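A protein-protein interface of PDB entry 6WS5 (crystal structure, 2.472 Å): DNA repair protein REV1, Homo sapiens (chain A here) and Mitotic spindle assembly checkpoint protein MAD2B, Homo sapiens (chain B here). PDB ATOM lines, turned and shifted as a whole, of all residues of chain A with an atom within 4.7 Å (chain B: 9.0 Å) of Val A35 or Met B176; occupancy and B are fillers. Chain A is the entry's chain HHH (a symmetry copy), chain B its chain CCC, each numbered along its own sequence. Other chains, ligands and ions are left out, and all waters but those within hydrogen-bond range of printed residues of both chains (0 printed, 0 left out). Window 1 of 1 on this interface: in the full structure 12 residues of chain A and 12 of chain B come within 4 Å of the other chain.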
ATOM      1  N   ILE A  31      10.461  10.657   9.653  1.00  0.00           N
ATOM      2  CA  ILE A  31      11.073  11.863  10.303  1.00  0.00           C
ATOM      3  C   ILE A  31       9.889  12.771  10.749  1.00  0.00           C
ATOM      4  O   ILE A  31       9.848  13.175  11.918  1.00  0.00           O
ATOM      5  CB  ILE A  31      12.095  12.522   9.378  1.00  0.00           C
ATOM      6  CG1 ILE A  31      13.214  11.561   9.011  1.00  0.00           C
ATOM      7  CG2 ILE A  31      12.689  13.795   9.917  1.00  0.00           C
ATOM      8  CD1 ILE A  31      14.249  12.149   8.045  1.00  0.00           C
ATOM      9  N   LEU A  32       8.869  12.966   9.911  1.00  0.00           N
ATOM     10  CA  LEU A  32       7.702  13.798  10.259  1.00  0.00           C
ATOM     11  C   LEU A  32       6.880  13.152  11.366  1.00  0.00           C
ATOM     12  O   LEU A  32       6.411  13.880  12.244  1.00  0.00           O
ATOM     13  CB  LEU A  32       6.874  13.978   8.991  1.00  0.00           C
ATOM     14  CG  LEU A  32       7.553  14.757   7.865  1.00  0.00           C
ATOM     15  CD1 LEU A  32       6.671  14.788   6.670  1.00  0.00           C
ATOM     16  CD2 LEU A  32       7.818  16.145   8.292  1.00  0.00           C
ATOM     17  N   GLN A  33       6.667  11.837  11.349  1.00  0.00           N
ATOM     18  CA  GLN A  33       5.967  11.097  12.438  1.00  0.00           C
ATOM     19  C   GLN A  33       6.642  11.356  13.809  1.00  0.00           C
ATOM     20  O   GLN A  33       5.938  11.401  14.896  1.00  0.00           O
ATOM     21  CB  GLN A  33       5.916   9.614  12.121  1.00  0.00           C
ATOM     22  CG  GLN A  33       5.094   8.788  13.091  1.00  0.00           C
ATOM     23  CD  GLN A  33       4.237   7.779  12.353  1.00  0.00           C
ATOM     24  OE1 GLN A  33       4.524   7.436  11.210  1.00  0.00           O
ATOM     25  NE2 GLN A  33       3.178   7.284  12.995  1.00  0.00           N
ATOM     26  N   VAL A  34       7.950  11.543  13.798  1.00  0.00           N
ATOM     27  CA  VAL A  34       8.765  11.776  15.021  1.00  0.00           C
ATOM     28  C   VAL A  34       8.583  13.254  15.457  1.00  0.00           C
ATOM     29  O   VAL A  34       8.426  13.504  16.698  1.00  0.00           O
ATOM     30  CB  VAL A  34      10.237  11.415  14.686  1.00  0.00           C
ATOM     31  CG1 VAL A  34      11.261  12.185  15.497  1.00  0.00           C
ATOM     32  CG2 VAL A  34      10.452   9.919  14.769  1.00  0.00           C
ATOM     33  N   VAL A  35       8.644  14.209  14.491  1.00  0.00           N
ATOM     34  CA  VAL A  35       8.305  15.638  14.716  1.00  0.00           C
ATOM     35  C   VAL A  35       6.914  15.718  15.391  1.00  0.00           C
ATOM     36  O   VAL A  35       6.830  16.387  16.417  1.00  0.00           O
ATOM     37  CB  VAL A  35       8.321  16.493  13.454  1.00  0.00           C
ATOM     38  CG1 VAL A  35       7.836  17.914  13.759  1.00  0.00           C
ATOM     39  CG2 VAL A  35       9.724  16.503  12.833  1.00  0.00           C
ATOM     40  N   LYS A  36       5.935  14.971  14.883  1.00  0.00           N
ATOM     41  CA  LYS A  36       4.563  14.974  15.438  1.00  0.00           C
ATOM     42  C   LYS A  36       4.584  14.412  16.863  1.00  0.00           C
ATOM     43  O   LYS A  36       3.989  15.076  17.777  1.00  0.00           O
ATOM     44  CB  LYS A  36       3.603  14.193  14.550  1.00  0.00           C
ATOM     45  CG  LYS A  36       2.278  13.849  15.181  1.00  0.00           C
ATOM     46  CD  LYS A  36       1.261  15.001  15.246  1.00  0.00           C
ATOM     47  CE  LYS A  36      -0.166  14.462  15.272  1.00  0.00           C
ATOM     48  NZ  LYS A  36      -0.977  15.105  16.322  1.00  0.00           N
ATOM     49  N   TYR A  37       5.211  13.258  17.083  1.00  0.00           N
ATOM     50  CA  TYR A  37       5.470  12.738  18.464  1.00  0.00           C
ATOM     51  C   TYR A  37       6.011  13.869  19.326  1.00  0.00           C
ATOM     52  O   TYR A  37       5.414  14.166  20.408  1.00  0.00           O
ATOM     53  CB  TYR A  37       6.467  11.558  18.454  1.00  0.00           C
ATOM     54  CG  TYR A  37       6.754  11.015  19.814  1.00  0.00           C
ATOM     55  CD1 TYR A  37       5.751  10.341  20.504  1.00  0.00           C
ATOM     56  CD2 TYR A  37       7.994  11.219  20.431  1.00  0.00           C
ATOM     57  CE1 TYR A  37       5.978   9.894  21.790  1.00  0.00           C
ATOM     58  CE2 TYR A  37       8.223  10.763  21.732  1.00  0.00           C
ATOM     59  CZ  TYR A  37       7.200  10.110  22.400  1.00  0.00           C
ATOM     60  OH  TYR A  37       7.351   9.674  23.691  1.00  0.00           O
ATOM     61  N   CYS A  38       7.043  14.578  18.854  1.00  0.00           N
ATOM     62  CA  CYS A  38       7.705  15.638  19.670  1.00  0.00           C
ATOM     63  C   CYS A  38       6.749  16.782  19.973  1.00  0.00           C
ATOM     64  O   CYS A  38       6.590  17.139  21.156  1.00  0.00           O
ATOM     65  CB  CYS A  38       8.980  16.165  19.018  1.00  0.00           C
ATOM     66  SG  CYS A  38      10.305  14.941  19.216  1.00  0.00           S
ATOM     67  N   THR A  39       6.105  17.312  18.940  1.00  0.00           N
ATOM     68  CA  THR A  39       5.175  18.453  19.090  1.00  0.00           C
ATOM     69  C   THR A  39       4.044  18.018  20.045  1.00  0.00           C
ATOM     70  O   THR A  39       3.646  18.865  20.888  1.00  0.00           O
ATOM     71  CB  THR A  39       4.752  19.031  17.747  1.00  0.00           C
ATOM     72  OG1 THR A  39       4.007  18.044  17.062  1.00  0.00           O
ATOM     73  CG2 THR A  39       5.928  19.509  16.929  1.00  0.00           C
ATOM     74  N   PHE A  75      16.665  18.964  11.278  1.00  0.00           N
ATOM     75  CA  PHE A  75      15.278  19.204  10.872  1.00  0.00           C
ATOM     76  C   PHE A  75      14.327  19.019  12.083  1.00  0.00           C
ATOM     77  O   PHE A  75      13.534  20.004  12.338  1.00  0.00           O
ATOM     78  CB  PHE A  75      14.880  18.264   9.746  1.00  0.00           C
ATOM     79  CG  PHE A  75      13.431  18.363   9.382  1.00  0.00           C
ATOM     80  CD1 PHE A  75      12.967  19.483   8.713  1.00  0.00           C
ATOM     81  CD2 PHE A  75      12.542  17.328   9.713  1.00  0.00           C
ATOM     82  CE1 PHE A  75      11.621  19.571   8.390  1.00  0.00           C
ATOM     83  CE2 PHE A  75      11.201  17.408   9.353  1.00  0.00           C
ATOM     84  CZ  PHE A  75      10.749  18.537   8.709  1.00  0.00           C
ATOM     85  N   ILE A  76      14.417  17.877  12.804  1.00  0.00           N
ATOM     86  CA  ILE A  76      13.581  17.575  13.996  1.00  0.00           C
ATOM     87  C   ILE A  76      13.716  18.740  15.006  1.00  0.00           C
ATOM     88  O   ILE A  76      12.712  19.302  15.403  1.00  0.00           O
ATOM     89  CB  ILE A  76      13.918  16.204  14.622  1.00  0.00           C
ATOM     90  CG1 ILE A  76      13.781  15.057  13.626  1.00  0.00           C
ATOM     91  CG2 ILE A  76      13.061  15.902  15.838  1.00  0.00           C
ATOM     92  CD1 ILE A  76      14.528  13.768  14.071  1.00  0.00           C
ATOM     93  N   ASN A  79      12.113  22.147  14.178  1.00  0.00           N
ATOM     94  CA  ASN A  79      10.643  22.103  14.271  1.00  0.00           C
ATOM     95  C   ASN A  79      10.225  22.154  15.738  1.00  0.00           C
ATOM     96  O   ASN A  79       9.258  22.886  16.099  1.00  0.00           O
ATOM     97  CB  ASN A  79      10.058  20.896  13.509  1.00  0.00           C
ATOM     98  CG  ASN A  79      10.034  21.181  12.016  1.00  0.00           C
ATOM     99  OD1 ASN A  79       9.401  22.138  11.608  1.00  0.00           O
ATOM    100  ND2 ASN A  79      10.753  20.403  11.196  1.00  0.00           N
ATOM    101  N   CYS B  86       2.763  31.699   3.774  1.00  0.00           N
ATOM    102  CA  CYS B  86       3.414  30.416   4.099  1.00  0.00           C
ATOM    103  C   CYS B  86       3.159  29.389   3.026  1.00  0.00           C
ATOM    104  O   CYS B  86       4.060  28.567   2.831  1.00  0.00           O
ATOM    105  CB  CYS B  86       2.974  29.848   5.437  1.00  0.00           C
ATOM    106  SG  CYS B  86       3.610  30.961   6.705  1.00  0.00           S
ATOM    107  N   PRO B  89       5.185  29.369  -1.259  1.00  0.00           N
ATOM    108  CA  PRO B  89       6.303  28.513  -1.652  1.00  0.00           C
ATOM    109  C   PRO B  89       5.899  27.105  -2.118  1.00  0.00           C
ATOM    110  O   PRO B  89       6.469  26.603  -3.061  1.00  0.00           O
ATOM    111  CB  PRO B  89       7.187  28.408  -0.379  1.00  0.00           C
ATOM    112  CG  PRO B  89       6.530  29.286   0.654  1.00  0.00           C
ATOM    113  CD  PRO B  89       5.538  30.172  -0.082  1.00  0.00           C
ATOM    114  N   LEU B  90       4.958  26.463  -1.418  1.00  0.00           N
ATOM    115  CA  LEU B  90       4.544  25.081  -1.740  1.00  0.00           C
ATOM    116  C   LEU B  90       3.825  25.031  -3.119  1.00  0.00           C
ATOM    117  O   LEU B  90       3.971  24.008  -3.826  1.00  0.00           O
ATOM    118  CB  LEU B  90       3.659  24.567  -0.617  1.00  0.00           C
ATOM    119  CG  LEU B  90       4.413  23.932   0.549  1.00  0.00           C
ATOM    120  CD1 LEU B  90       5.227  24.970   1.222  1.00  0.00           C
ATOM    121  CD2 LEU B  90       3.466  23.221   1.529  1.00  0.00           C
ATOM    122  N   ASP B  95       3.301  21.486  -4.870  1.00  0.00           N
ATOM    123  CA  ASP B  95       3.502  20.442  -3.800  1.00  0.00           C
ATOM    124  C   ASP B  95       2.189  20.159  -3.037  1.00  0.00           C
ATOM    125  O   ASP B  95       2.143  19.251  -2.188  1.00  0.00           O
ATOM    126  CB  ASP B  95       4.568  20.891  -2.783  1.00  0.00           C
ATOM    127  CG  ASP B  95       6.033  20.595  -3.128  1.00  0.00           C
ATOM    128  OD1 ASP B  95       6.258  19.717  -4.016  1.00  0.00           O
ATOM    129  OD2 ASP B  95       6.955  21.202  -2.477  1.00  0.00           O
ATOM    130  N   THR B 168      -0.475  18.153   1.305  1.00  0.00           N
ATOM    131  CA  THR B 168       0.630  18.039   0.290  1.00  0.00           C
ATOM    132  C   THR B 168       0.510  16.692  -0.452  1.00  0.00           C
ATOM    133  O   THR B 168       0.003  15.727   0.169  1.00  0.00           O
ATOM    134  CB  THR B 168       2.033  18.070   0.933  1.00  0.00           C
ATOM    135  OG1 THR B 168       2.065  17.139   2.071  1.00  0.00           O
ATOM    136  CG2 THR B 168       2.439  19.482   1.296  1.00  0.00           C
ATOM    137  N   GLU B 170       2.973  14.387  -1.484  1.00  0.00           N
ATOM    138  CA  GLU B 170       3.605  13.354  -0.607  1.00  0.00           C
ATOM    139  C   GLU B 170       4.209  14.054   0.629  1.00  0.00           C
ATOM    140  O   GLU B 170       4.523  15.271   0.585  1.00  0.00           O
ATOM    141  CB  GLU B 170       4.611  12.497  -1.409  1.00  0.00           C
ATOM    142  CG  GLU B 170       5.934  13.175  -1.761  1.00  0.00           C
ATOM    143  CD  GLU B 170       6.039  13.905  -3.086  1.00  0.00           C
ATOM    144  OE1 GLU B 170       7.200  14.269  -3.464  1.00  0.00           O
ATOM    145  OE2 GLU B 170       4.978  14.119  -3.741  1.00  0.00           O
ATOM    146  N   ALA B 171       4.328  13.328   1.726  1.00  0.00           N
ATOM    147  CA  ALA B 171       5.041  13.718   2.949  1.00  0.00           C
ATOM    148  C   ALA B 171       6.546  13.947   2.664  1.00  0.00           C
ATOM    149  O   ALA B 171       7.196  13.123   2.144  1.00  0.00           O
ATOM    150  CB  ALA B 171       4.805  12.648   4.006  1.00  0.00           C
ATOM    151  N   ALA B 172       7.057  15.107   3.028  1.00  0.00           N
ATOM    152  CA  ALA B 172       8.391  15.579   2.678  1.00  0.00           C
ATOM    153  C   ALA B 172       8.788  16.692   3.651  1.00  0.00           C
ATOM    154  O   ALA B 172       8.014  17.657   3.818  1.00  0.00           O
ATOM    155  CB  ALA B 172       8.405  16.054   1.257  1.00  0.00           C
ATOM    156  N   THR B 173       9.945  16.535   4.287  1.00  0.00           N
ATOM    157  CA  THR B 173      10.574  17.585   5.099  1.00  0.00           C
ATOM    158  C   THR B 173      10.687  18.881   4.299  1.00  0.00           C
ATOM    159  O   THR B 173      10.498  19.961   4.939  1.00  0.00           O
ATOM    160  CB  THR B 173      11.898  17.079   5.668  1.00  0.00           C
ATOM    161  OG1 THR B 173      12.732  16.838   4.563  1.00  0.00           O
ATOM    162  CG2 THR B 173      11.734  15.800   6.466  1.00  0.00           C
ATOM    163  N   ARG B 174      10.975  18.835   2.993  1.00  0.00           N
ATOM    164  CA  ARG B 174      11.172  20.100   2.213  1.00  0.00           C
ATOM    165  C   ARG B 174       9.903  20.958   2.375  1.00  0.00           C
ATOM    166  O   ARG B 174      10.046  22.166   2.593  1.00  0.00           O
ATOM    167  CB  ARG B 174      11.600  19.891   0.763  1.00  0.00           C
ATOM    168  CG  ARG B 174      10.556  19.217  -0.100  1.00  0.00           C
ATOM    169  CD  ARG B 174      10.921  18.997  -1.557  1.00  0.00           C
ATOM    170  NE  ARG B 174       9.762  18.452  -2.262  1.00  0.00           N
ATOM    171  CZ  ARG B 174       9.450  17.146  -2.333  1.00  0.00           C
ATOM    172  NH1 ARG B 174      10.248  16.247  -1.780  1.00  0.00           N
ATOM    173  NH2 ARG B 174       8.351  16.741  -2.973  1.00  0.00           N
ATOM    174  N   ASN B 175       8.714  20.345   2.435  1.00  0.00           N
ATOM    175  CA  ASN B 175       7.419  21.036   2.707  1.00  0.00           C
ATOM    176  C   ASN B 175       7.456  21.810   4.028  1.00  0.00           C
ATOM    177  O   ASN B 175       7.219  23.060   4.020  1.00  0.00           O
ATOM    178  CB  ASN B 175       6.220  20.063   2.597  1.00  0.00           C
ATOM    179  CG  ASN B 175       6.075  19.525   1.183  1.00  0.00           C
ATOM    180  OD1 ASN B 175       6.394  20.289   0.232  1.00  0.00           O
ATOM    181  ND2 ASN B 175       5.612  18.262   1.074  1.00  0.00           N
ATOM    182  N   MET B 176       7.808  21.146   5.135  1.00  0.00           N
ATOM    183  CA  MET B 176       7.826  21.792   6.478  1.00  0.00           C
ATOM    184  C   MET B 176       8.917  22.816   6.550  1.00  0.00           C
ATOM    185  O   MET B 176       8.703  23.790   7.281  1.00  0.00           O
ATOM    186  CB  MET B 176       7.977  20.777   7.608  1.00  0.00           C
ATOM    187  CG  MET B 176       6.631  20.200   7.975  1.00  0.00           C
ATOM    188  SD  MET B 176       6.576  19.245   9.441  1.00  0.00           S
ATOM    189  CE  MET B 176       7.426  20.288  10.608  1.00  0.00           C
ATOM    190  N   GLU B 177       9.998  22.713   5.768  1.00  0.00           N
ATOM    191  CA  GLU B 177      11.002  23.811   5.860  1.00  0.00           C
ATOM    192  C   GLU B 177      10.557  24.945   4.949  1.00  0.00           C
ATOM    193  O   GLU B 177      10.810  26.098   5.329  1.00  0.00           O
ATOM    194  CB  GLU B 177      12.453  23.336   5.737  1.00  0.00           C
ATOM    195  CG  GLU B 177      12.782  22.608   4.459  1.00  0.00           C
ATOM    196  CD  GLU B 177      14.151  21.933   4.491  1.00  0.00           C
ATOM    197  OE1 GLU B 177      14.700  21.701   5.641  1.00  0.00           O
ATOM    198  OE2 GLU B 177      14.632  21.575   3.347  1.00  0.00           O
ATOM    199  N   LYS B 178       9.816  24.690   3.871  1.00  0.00           N
ATOM    200  CA  LYS B 178       9.358  25.795   2.968  1.00  0.00           C
ATOM    201  C   LYS B 178       8.222  26.631   3.635  1.00  0.00           C
ATOM    202  O   LYS B 178       8.167  27.873   3.380  1.00  0.00           O
ATOM    203  CB  LYS B 178       9.015  25.218   1.597  1.00  0.00           C
ATOM    204  CG  LYS B 178      10.201  24.559   0.872  1.00  0.00           C
ATOM    205  CD  LYS B 178      10.309  24.843  -0.624  1.00  0.00           C
ATOM    206  CE  LYS B 178       9.105  24.375  -1.435  1.00  0.00           C
ATOM    207  NZ  LYS B 178       8.770  22.944  -1.184  1.00  0.00           N
ATOM    208  N   ILE B 179       7.356  26.036   4.462  1.00  0.00           N
ATOM    209  CA  ILE B 179       6.219  26.778   5.102  1.00  0.00           C
ATOM    210  C   ILE B 179       6.647  27.562   6.343  1.00  0.00           C
ATOM    211  O   ILE B 179       5.913  28.546   6.639  1.00  0.00           O
ATOM    212  CB  ILE B 179       5.084  25.856   5.500  1.00  0.00           C
ATOM    213  CG1 ILE B 179       5.613  24.722   6.344  1.00  0.00           C
ATOM    214  CG2 ILE B 179       4.305  25.337   4.311  1.00  0.00           C
ATOM    215  CD1 ILE B 179       5.106  24.803   7.734  1.00  0.00           C
ATOM    216  N   GLN B 180       7.701  27.123   7.068  1.00  0.00           N
ATOM    217  CA  GLN B 180       8.104  27.739   8.365  1.00  0.00           C
ATOM    218  C   GLN B 180       8.860  29.004   8.052  1.00  0.00           C
ATOM    219  O   GLN B 180       9.903  29.212   8.660  1.00  0.00           O
ATOM    220  CB  GLN B 180       8.954  26.806   9.254  1.00  0.00           C
ATOM    221  CG  GLN B 180       8.305  25.442   9.624  1.00  0.00           C
ATOM    222  CD  GLN B 180       7.233  25.428  10.699  1.00  0.00           C
ATOM    223  OE1 GLN B 180       6.597  26.420  11.078  1.00  0.00           O
ATOM    224  NE2 GLN B 180       6.983  24.258  11.211  1.00  0.00           N
ATOM    225  N   VAL B 181       8.363  29.826   7.127  1.00  0.00           N
ATOM    226  CA  VAL B 181       9.003  31.124   6.774  1.00  0.00           C
ATOM    227  C   VAL B 181       8.560  32.154   7.835  1.00  0.00           C
ATOM    228  O   VAL B 181       9.435  32.487   8.667  1.00  0.00           O
ATOM    229  CB  VAL B 181       8.702  31.532   5.317  1.00  0.00           C
ATOM    230  CG1 VAL B 181       7.243  31.940   5.063  1.00  0.00           C
ATOM    231  CG2 VAL B 181       9.671  32.601   4.836  1.00  0.00           C
ATOM    232  N   ILE B 182       7.270  32.571   7.876  1.00  0.00           N
ATOM    233  CA  ILE B 182       6.753  33.703   8.724  1.00  0.00           C
ATOM    234  C   ILE B 182       6.967  33.404  10.214  1.00  0.00           C
ATOM    235  O   ILE B 182       6.639  32.296  10.638  1.00  0.00           O
ATOM    236  CB  ILE B 182       5.274  34.039   8.498  1.00  0.00           C
ATOM    237  CG1 ILE B 182       5.042  34.861   7.232  1.00  0.00           C
ATOM    238  CG2 ILE B 182       4.714  34.795   9.702  1.00  0.00           C
ATOM    239  CD1 ILE B 182       3.591  35.205   7.034  1.00  0.00           C
ATOM    240  N   PHE B 185       4.465  32.497  13.626  1.00  0.00           N
ATOM    241  CA  PHE B 185       3.433  31.756  12.863  1.00  0.00           C
ATOM    242  C   PHE B 185       3.925  30.378  12.443  1.00  0.00           C
ATOM    243  O   PHE B 185       3.808  30.010  11.302  1.00  0.00           O
ATOM    244  CB  PHE B 185       2.933  32.494  11.618  1.00  0.00           C
ATOM    245  CG  PHE B 185       1.540  32.078  11.199  1.00  0.00           C
ATOM    246  CD1 PHE B 185       0.433  32.578  11.859  1.00  0.00           C
ATOM    247  CD2 PHE B 185       1.347  31.202  10.130  1.00  0.00           C
ATOM    248  CE1 PHE B 185      -0.857  32.199  11.453  1.00  0.00           C
ATOM    249  CE2 PHE B 185       0.074  30.826   9.722  1.00  0.00           C
ATOM    250  CZ  PHE B 185      -1.048  31.312  10.412  1.00  0.00           C
ATOM    251  N   PRO B 186       4.298  29.478  13.374  1.00  0.00           N
ATOM    252  CA  PRO B 186       4.717  28.142  12.969  1.00  0.00           C
ATOM    253  C   PRO B 186       3.572  27.195  12.586  1.00  0.00           C
ATOM    254  O   PRO B 186       2.407  27.433  12.845  1.00  0.00           O
ATOM    255  CB  PRO B 186       5.385  27.662  14.253  1.00  0.00           C
ATOM    256  CG  PRO B 186       4.481  28.256  15.318  1.00  0.00           C
ATOM    257  CD  PRO B 186       4.235  29.660  14.826  1.00  0.00           C
ATOM    258  N   TRP B 187       3.978  26.097  11.986  1.00  0.00           N
ATOM    259  CA  TRP B 187       3.113  25.067  11.389  1.00  0.00           C
ATOM    260  C   TRP B 187       3.377  23.732  12.072  1.00  0.00           C
ATOM    261  O   TRP B 187       4.499  23.546  12.566  1.00  0.00           O
ATOM    262  CB  TRP B 187       3.387  25.055   9.890  1.00  0.00           C
ATOM    263  CG  TRP B 187       2.765  26.191   9.111  1.00  0.00           C
ATOM    264  CD1 TRP B 187       3.233  27.484   8.963  1.00  0.00           C
ATOM    265  CD2 TRP B 187       1.524  26.147   8.403  1.00  0.00           C
ATOM    266  NE1 TRP B 187       2.386  28.218   8.188  1.00  0.00           N
ATOM    267  CE2 TRP B 187       1.322  27.420   7.837  1.00  0.00           C
ATOM    268  CE3 TRP B 187       0.606  25.122   8.150  1.00  0.00           C
ATOM    269  CZ2 TRP B 187       0.201  27.706   7.049  1.00  0.00           C
ATOM    270  CZ3 TRP B 187      -0.451  25.372   7.310  1.00  0.00           C
ATOM    271  CH2 TRP B 187      -0.662  26.655   6.801  1.00  0.00           C
ATOM    272  N   ILE B 188       2.331  22.886  12.183  1.00  0.00           N
ATOM    273  CA  ILE B 188       2.463  21.499  12.752  1.00  0.00           C
ATOM    274  C   ILE B 188       1.692  20.526  11.835  1.00  0.00           C
ATOM    275  O   ILE B 188       0.912  20.964  10.928  1.00  0.00           O
ATOM    276  CB  ILE B 188       1.975  21.412  14.197  1.00  0.00           C
ATOM    277  CG1 ILE B 188       0.452  21.689  14.331  1.00  0.00           C
ATOM    278  CG2 ILE B 188       2.835  22.276  15.125  1.00  0.00           C
ATOM    279  CD1 ILE B 188      -0.084  21.648  15.713  1.00  0.00           C
ATOM    280  N   LEU B 189       1.967  19.256  12.039  1.00  0.00           N
ATOM    281  CA  LEU B 189       1.260  18.122  11.418  1.00  0.00           C
ATOM    282  C   LEU B 189      -0.073  17.977  12.164  1.00  0.00           C
ATOM    283  O   LEU B 189      -0.095  17.971  13.424  1.00  0.00           O
ATOM    284  CB  LEU B 189       2.163  16.886  11.507  1.00  0.00           C
ATOM    285  CG  LEU B 189       3.354  16.995  10.548  1.00  0.00           C
ATOM    286  CD1 LEU B 189       4.519  16.155  10.959  1.00  0.00           C
ATOM    287  CD2 LEU B 189       2.972  16.632   9.141  1.00  0.00           C
ATOM    288  N   ALA B 190      -1.163  17.926  11.424  1.00  0.00           N
ATOM    289  CA  ALA B 190      -2.512  18.089  12.004  1.00  0.00           C
ATOM    290  C   ALA B 190      -2.753  16.800  12.762  1.00  0.00           C
ATOM    291  O   ALA B 190      -2.108  15.819  12.380  1.00  0.00           O
ATOM    292  CB  ALA B 190      -3.528  18.352  10.914  1.00  0.00           C
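The side-chain amide oxygen (OD1) of Asn A79 sits at hydrogen-bond distance from the side-chain amide nitrogen (NE2) of Gln B180, 3.2 Å away.
Val A35 touches just one residue of chain B: Met B176 (3.97 Å).
Of chain A, only Leu A32, Val A35, Phe A75 and Asn A79 come within 4 Å of Met B176.
No residue of chain B comes within 4 Å of Val A34.
Of the printed residues of chain A, Thr B173 touches Phe A75 (3.3 Å).
Printed residues of chain A within 4 Å of Ala B190: Lys A36 (3.7 Å).
Printed residues of chain A within 4 Å of Ala B172: Leu A32 (3.7 Å).
Printed residues of chain B within 4 Å of Asn A79: Met B176 (2.9 Å) and Gln B180 (3.2 Å).
Printed residues of chain B within 4 Å of Leu A32: Ala B171 (3.9 Å), Ala B172 (3.7 Å), Met B176 (3.5 Å) and Leu B189 (3.2 Å).
Pro B89 touches none of the printed residues of chain A.
The nearest printed residue of chain A that does not touch Met B176 is Thr A39 (6.5 Å).
Among the printed residues, pairs that only touch across the chains: Asn A79 with Met B176, Leu A32 with Leu B189, Phe A75 with Thr B173, Leu A32 with Met B176, Leu A32 with Ala B172, Phe A75 with Met B176, Lys A36 with Ala B190, Lys A36 with Leu B189, Leu A32 with Ala B171 and Val A35 with Met B176.
Of the 24 printed residues of chain B, 7 touch a printed residue of chain A.
Hydrophobic or aromatic side chains of chain B within 4 Å of the printed part of chain A: Ala B171, Met B176 and Leu B189.
Of the 12 printed residues of chain A, 5 touch a printed residue of chain B.
Hydrophobic or aromatic side chains of chain A that line the printed part of chain B: Leu A32, Val A35 and Phe A75.
Among the printed residues, 11 pairs touch across the chains.
The side-chain amide nitrogen of Asn A79 is in hydrogen-bond range of the backbone carbonyl oxygen of Phe A75, at 3.0 Å.
The side-chain amide oxygen of Gln B180 sits at hydrogen-bond distance from the backbone NH of Trp B187, 2.8 Å away.
The side-chain hydroxyl (OG1) of Thr A39 lies close to the backbone carbonyl oxygen (O) of Val A35 (3.3 Å).
The backbone carbonyl oxygen (O) of Lys A36 sits at hydrogen-bond distance from the side-chain hydroxyl (OG1) of Thr A39 (3.1 Å).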
